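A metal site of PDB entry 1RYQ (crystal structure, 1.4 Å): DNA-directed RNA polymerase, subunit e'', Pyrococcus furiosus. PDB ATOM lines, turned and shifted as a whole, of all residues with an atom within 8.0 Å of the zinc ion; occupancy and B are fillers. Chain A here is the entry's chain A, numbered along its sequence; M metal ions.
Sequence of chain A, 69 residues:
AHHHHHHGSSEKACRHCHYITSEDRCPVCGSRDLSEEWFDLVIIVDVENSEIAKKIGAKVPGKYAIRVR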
ATOM      1  N   ALA A  13     -16.434   6.243  25.917  1.00  0.00           N
ATOM      2  CA  ALA A  13     -16.805   6.922  24.678  1.00  0.00           C
ATOM      3  C   ALA A  13     -17.703   8.116  25.002  1.00  0.00           C
ATOM      4  O   ALA A  13     -18.609   8.029  25.842  1.00  0.00           O
ATOM      5  CB  ALA A  13     -17.544   5.982  23.790  1.00  0.00           C
ATOM      6  N   CYS A  14     -17.468   9.211  24.291  1.00  0.00           N
ATOM      7  CA  CYS A  14     -18.282  10.398  24.474  1.00  0.00           C
ATOM      8  C   CYS A  14     -19.711  10.189  23.941  1.00  0.00           C
ATOM      9  O   CYS A  14     -19.887   9.779  22.783  1.00  0.00           O
ATOM     10  CB  CYS A  14     -17.616  11.552  23.747  1.00  0.00           C
ATOM     11  SG  CYS A  14     -18.575  13.093  23.861  1.00  0.00           S
ATOM     12  N   ARG A  15     -20.695  10.503  24.761  1.00  0.00           N
ATOM     13  CA  ARG A  15     -22.073  10.364  24.340  1.00  0.00           C
ATOM     14  C   ARG A  15     -22.501  11.350  23.256  1.00  0.00           C
ATOM     15  O   ARG A  15     -23.527  11.123  22.590  1.00  0.00           O
ATOM     16  CB  ARG A  15     -22.994  10.494  25.544  1.00  0.00           C
ATOM     17  CG  ARG A  15     -22.926   9.282  26.470  1.00  0.00           C
ATOM     18  CD  ARG A  15     -23.692   9.442  27.784  1.00  0.00           C
ATOM     19  NE  ARG A  15     -24.001   8.115  28.355  1.00  0.00           N
ATOM     20  CZ  ARG A  15     -23.674   7.716  29.578  1.00  0.00           C
ATOM     21  NH1 ARG A  15     -23.031   8.530  30.433  1.00  0.00           N
ATOM     22  NH2 ARG A  15     -23.992   6.469  29.952  1.00  0.00           N
ATOM     23  N   HIS A  16     -21.735  12.412  23.014  1.00  0.00           N
ATOM     24  CA  HIS A  16     -22.107  13.420  22.031  1.00  0.00           C
ATOM     25  C   HIS A  16     -21.382  13.282  20.699  1.00  0.00           C
ATOM     26  O   HIS A  16     -21.995  13.484  19.651  1.00  0.00           O
ATOM     27  CB  HIS A  16     -21.940  14.818  22.641  1.00  0.00           C
ATOM     28  CG  HIS A  16     -22.703  14.957  23.912  1.00  0.00           C
ATOM     29  ND1 HIS A  16     -24.070  15.108  23.949  1.00  0.00           N
ATOM     30  CD2 HIS A  16     -22.283  14.871  25.205  1.00  0.00           C
ATOM     31  CE1 HIS A  16     -24.462  15.132  25.211  1.00  0.00           C
ATOM     32  NE2 HIS A  16     -23.395  14.961  25.994  1.00  0.00           N
ATOM     33  N   CYS A  17     -20.093  12.931  20.725  1.00  0.00           N
ATOM     34  CA  CYS A  17     -19.342  12.851  19.460  1.00  0.00           C
ATOM     35  C   CYS A  17     -18.707  11.470  19.273  1.00  0.00           C
ATOM     36  O   CYS A  17     -18.099  11.266  18.235  1.00  0.00           O
ATOM     37  CB  CYS A  17     -18.273  13.955  19.379  1.00  0.00           C
ATOM     38  SG  CYS A  17     -16.809  13.626  20.417  1.00  0.00           S
ATOM     39  N   HIS A  18     -18.838  10.580  20.244  1.00  0.00           N
ATOM     40  CA  HIS A  18     -18.382   9.192  20.136  1.00  0.00           C
ATOM     41  C   HIS A  18     -16.875   8.944  20.171  1.00  0.00           C
ATOM     42  O   HIS A  18     -16.445   7.798  20.041  1.00  0.00           O
ATOM     43  CB  HIS A  18     -19.010   8.482  18.916  1.00  0.00           C
ATOM     44  CG  HIS A  18     -20.495   8.282  19.025  1.00  0.00           C
ATOM     45  ND1 HIS A  18     -21.127   7.251  18.375  1.00  0.00           N
ATOM     46  CD2 HIS A  18     -21.440   8.896  19.779  1.00  0.00           C
ATOM     47  CE1 HIS A  18     -22.428   7.286  18.650  1.00  0.00           C
ATOM     48  NE2 HIS A  18     -22.642   8.262  19.501  1.00  0.00           N
ATOM     49  N   TYR A  19     -16.086   9.967  20.464  1.00  0.00           N
ATOM     50  CA  TYR A  19     -14.646   9.773  20.588  1.00  0.00           C
ATOM     51  C   TYR A  19     -14.360   8.942  21.818  1.00  0.00           C
ATOM     52  O   TYR A  19     -15.041   9.074  22.866  1.00  0.00           O
ATOM     53  CB  TYR A  19     -14.013  11.149  20.733  1.00  0.00           C
ATOM     54  CG  TYR A  19     -12.507  11.195  20.751  1.00  0.00           C
ATOM     55  CD1 TYR A  19     -11.798  11.296  19.572  1.00  0.00           C
ATOM     56  CD2 TYR A  19     -11.824  11.198  21.962  1.00  0.00           C
ATOM     57  CE1 TYR A  19     -10.380  11.411  19.612  1.00  0.00           C
ATOM     58  CE2 TYR A  19     -10.424  11.286  22.020  1.00  0.00           C
ATOM     59  CZ  TYR A  19      -9.749  11.378  20.861  1.00  0.00           C
ATOM     60  OH  TYR A  19      -8.351  11.453  20.930  1.00  0.00           O
ATOM     61  N   ILE A  20     -13.350   8.081  21.701  1.00  0.00           N
ATOM     62  CA  ILE A  20     -12.960   7.213  22.832  1.00  0.00           C
ATOM     63  C   ILE A  20     -11.713   7.748  23.520  1.00  0.00           C
ATOM     64  O   ILE A  20     -10.715   8.033  22.838  1.00  0.00           O
ATOM     65  CB  ILE A  20     -12.754   5.771  22.346  1.00  0.00           C
ATOM     66  CG1 ILE A  20     -14.059   5.138  21.858  1.00  0.00           C
ATOM     67  CG2 ILE A  20     -12.200   4.897  23.489  1.00  0.00           C
ATOM     68  CD1 ILE A  20     -13.846   3.836  21.067  1.00  0.00           C
ATOM     69  N   THR A  21     -11.799   7.934  24.842  1.00  0.00           N
ATOM     70  CA  THR A  21     -10.720   8.543  25.618  1.00  0.00           C
ATOM     71  C   THR A  21     -10.606   7.877  26.990  1.00  0.00           C
ATOM     72  O   THR A  21     -11.568   7.328  27.502  1.00  0.00           O
ATOM     73  CB  THR A  21     -10.976  10.072  25.742  1.00  0.00           C
ATOM     74  OG1 THR A  21      -9.874  10.710  26.410  1.00  0.00           O
ATOM     75  CG2 THR A  21     -12.147  10.386  26.647  1.00  0.00           C
ATOM     76  N   ARG A  25     -12.651  13.992  30.386  1.00  0.00           N
ATOM     77  CA  ARG A  25     -13.535  14.738  29.495  1.00  0.00           C
ATOM     78  C   ARG A  25     -13.095  14.502  28.065  1.00  0.00           C
ATOM     79  O   ARG A  25     -11.947  14.204  27.781  1.00  0.00           O
ATOM     80  CB  ARG A  25     -13.610  16.219  29.878  1.00  0.00           C
ATOM     81  CG  ARG A  25     -12.600  17.160  29.275  1.00  0.00           C
ATOM     82  CD  ARG A  25     -12.377  18.435  30.103  1.00  0.00           C
ATOM     83  NE  ARG A  25     -13.602  18.944  30.706  1.00  0.00           N
ATOM     84  CZ  ARG A  25     -13.647  19.676  31.812  1.00  0.00           C
ATOM     85  NH2 ARG A  25     -14.813  20.107  32.301  1.00  0.00           N
ATOM     86  N   CYS A  26     -14.047  14.605  27.146  1.00  0.00           N
ATOM     87  CA  CYS A  26     -13.777  14.382  25.757  1.00  0.00           C
ATOM     88  C   CYS A  26     -12.893  15.496  25.195  1.00  0.00           C
ATOM     89  O   CYS A  26     -13.285  16.677  25.283  1.00  0.00           O
ATOM     90  CB  CYS A  26     -15.094  14.413  25.015  1.00  0.00           C
ATOM     91  SG  CYS A  26     -14.893  14.166  23.244  1.00  0.00           S
ATOM     92  N   PRO A  27     -11.735  15.165  24.597  1.00  0.00           N
ATOM     93  CA  PRO A  27     -10.892  16.210  24.000  1.00  0.00           C
ATOM     94  C   PRO A  27     -11.476  16.850  22.748  1.00  0.00           C
ATOM     95  O   PRO A  27     -11.092  17.964  22.391  1.00  0.00           O
ATOM     96  CB  PRO A  27      -9.584  15.482  23.641  1.00  0.00           C
ATOM     97  CG  PRO A  27      -9.723  14.108  24.057  1.00  0.00           C
ATOM     98  CD  PRO A  27     -11.113  13.831  24.548  1.00  0.00           C
ATOM     99  N   VAL A  28     -12.421  16.160  22.100  1.00  0.00           N
ATOM    100  CA  VAL A  28     -12.971  16.668  20.850  1.00  0.00           C
ATOM    101  C   VAL A  28     -14.027  17.764  21.089  1.00  0.00           C
ATOM    102  O   VAL A  28     -13.863  18.896  20.612  1.00  0.00           O
ATOM    103  CB  VAL A  28     -13.547  15.521  19.986  1.00  0.00           C
ATOM    104  CG1 VAL A  28     -14.210  16.067  18.743  1.00  0.00           C
ATOM    105  CG2 VAL A  28     -12.412  14.564  19.600  1.00  0.00           C
ATOM    106  N   CYS A  29     -15.060  17.452  21.861  1.00  0.00           N
ATOM    107  CA  CYS A  29     -16.163  18.403  22.079  1.00  0.00           C
ATOM    108  C   CYS A  29     -16.129  19.011  23.462  1.00  0.00           C
ATOM    109  O   CYS A  29     -16.905  19.926  23.751  1.00  0.00           O
ATOM    110  CB  CYS A  29     -17.501  17.702  21.806  1.00  0.00           C
ATOM    111  SG  CYS A  29     -17.991  16.473  23.069  1.00  0.00           S
ATOM    112  N   GLY A  30     -15.293  18.485  24.366  1.00  0.00           N
ATOM    113  CA  GLY A  30     -15.239  19.003  25.744  1.00  0.00           C
ATOM    114  C   GLY A  30     -16.200  18.364  26.734  1.00  0.00           C
ATOM    115  O   GLY A  30     -16.133  18.676  27.908  1.00  0.00           O
ATOM    116  N   SER A  31     -17.107  17.478  26.303  1.00  0.00           N
ATOM    117  CA  SER A  31     -18.107  16.957  27.220  1.00  0.00           C
ATOM    118  C   SER A  31     -17.533  16.054  28.321  1.00  0.00           C
ATOM    119  O   SER A  31     -16.559  15.290  28.088  1.00  0.00           O
ATOM    120  CB  SER A  31     -19.173  16.158  26.462  1.00  0.00           C
ATOM    121  OG  SER A  31     -20.136  15.593  27.322  1.00  0.00           O
ATOM    122  N   ARG A  32     -18.196  16.069  29.468  1.00  0.00           N
ATOM    123  CA  ARG A  32     -17.896  15.126  30.535  1.00  0.00           C
ATOM    124  C   ARG A  32     -18.766  13.867  30.445  1.00  0.00           C
ATOM    125  O   ARG A  32     -18.630  12.943  31.248  1.00  0.00           O
ATOM    126  CB  ARG A  32     -18.209  15.795  31.865  1.00  0.00           C
ATOM    127  CG  ARG A  32     -17.370  17.013  32.185  1.00  0.00           C
ATOM    128  CD  ARG A  32     -17.734  17.576  33.542  1.00  0.00           C
ATOM    129  NE  ARG A  32     -17.234  18.913  33.826  1.00  0.00           N
ATOM    130  CZ  ARG A  32     -17.013  19.403  35.053  1.00  0.00           C
ATOM    131  NH1 ARG A  32     -17.266  18.653  36.118  1.00  0.00           N
ATOM    132  NH2 ARG A  32     -16.560  20.642  35.218  1.00  0.00           N
ATOM    133  N   ASP A  33     -19.624  13.774  29.441  1.00  0.00           N
ATOM    134  CA  ASP A  33     -20.538  12.650  29.333  1.00  0.00           C
ATOM    135  C   ASP A  33     -19.901  11.428  28.643  1.00  0.00           C
ATOM    136  O   ASP A  33     -20.240  11.062  27.491  1.00  0.00           O
ATOM    137  CB  ASP A  33     -21.812  13.060  28.584  1.00  0.00           C
ATOM    138  CG  ASP A  33     -22.696  13.979  29.390  1.00  0.00           C
ATOM    139  OD1 ASP A  33     -22.773  13.784  30.625  1.00  0.00           O
ATOM    140  OD2 ASP A  33     -23.373  14.848  28.834  1.00  0.00           O
ATOM    141  N   LEU A  34     -19.002  10.793  29.388  1.00  0.00           N
ATOM    142  CA  LEU A  34     -18.241   9.648  28.898  1.00  0.00           C
ATOM    143  C   LEU A  34     -18.906   8.376  29.397  1.00  0.00           C
ATOM    144  O   LEU A  34     -19.147   8.243  30.604  1.00  0.00           O
ATOM    145  CB  LEU A  34     -16.807   9.738  29.369  1.00  0.00           C
ATOM    146  CG  LEU A  34     -16.055  11.009  28.994  1.00  0.00           C
ATOM    147  CD1 LEU A  34     -14.640  11.008  29.534  1.00  0.00           C
ATOM    148  CD2 LEU A  34     -15.998  11.166  27.452  1.00  0.00           C
ATOM    149  N   TYR A  64     -12.975   6.046  17.721  1.00  0.00           N
ATOM    150  CA  TYR A  64     -14.401   6.355  17.886  1.00  0.00           C
ATOM    151  C   TYR A  64     -15.209   5.085  18.032  1.00  0.00           C
ATOM    152  O   TYR A  64     -14.846   4.034  17.456  1.00  0.00           O
ATOM    153  CB  TYR A  64     -14.932   7.142  16.687  1.00  0.00           C
ATOM    154  CG  TYR A  64     -14.453   8.543  16.587  1.00  0.00           C
ATOM    155  CD1 TYR A  64     -15.239   9.612  17.044  1.00  0.00           C
ATOM    156  CD2 TYR A  64     -13.210   8.817  16.009  1.00  0.00           C
ATOM    157  CE1 TYR A  64     -14.767  10.912  16.929  1.00  0.00           C
ATOM    158  CE2 TYR A  64     -12.746  10.115  15.900  1.00  0.00           C
ATOM    159  CZ  TYR A  64     -13.539  11.154  16.392  1.00  0.00           C
ATOM    160  OH  TYR A  64     -13.090  12.461  16.282  1.00  0.00           O
HETATM  161 ZN    ZN M   1     -17.139  14.423  22.544  1.00  0.00          ZN
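The zinc ion is bound by SG of Cys 29 (2.3 Å), SG of Cys 17 (2.3 Å), SG of Cys 14 (2.4 Å) and SG of Cys 26 (2.4 Å).
SG of Cys 26 lies close to N of Val 28, at 3.4 Å.
The backbone NH (N) of Ser 31 sits close to the side-chain sulfur (SG) of Cys 29 (3.5 Å).
N of Cys 26 sits at hydrogen-bond distance from O of Ser 31, at 2.8 Å.
The side-chain sulfur (SG) of Cys 17 sits close to the backbone NH (N) of Tyr 19, at 3.7 Å.
The backbone NH (N) of His 16 lies close to the side-chain sulfur (SG) of Cys 14 (3.3 Å).
O of Tyr 19 is in hydrogen-bond range of N of Cys 14 (2.8 Å).
Within 4 Å of the zinc ion: Cys 14, Cys 17, Cys 26 and Cys 29.
The nearest printed residue that does not touch the zinc ion is Val 28 (4.5 Å).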
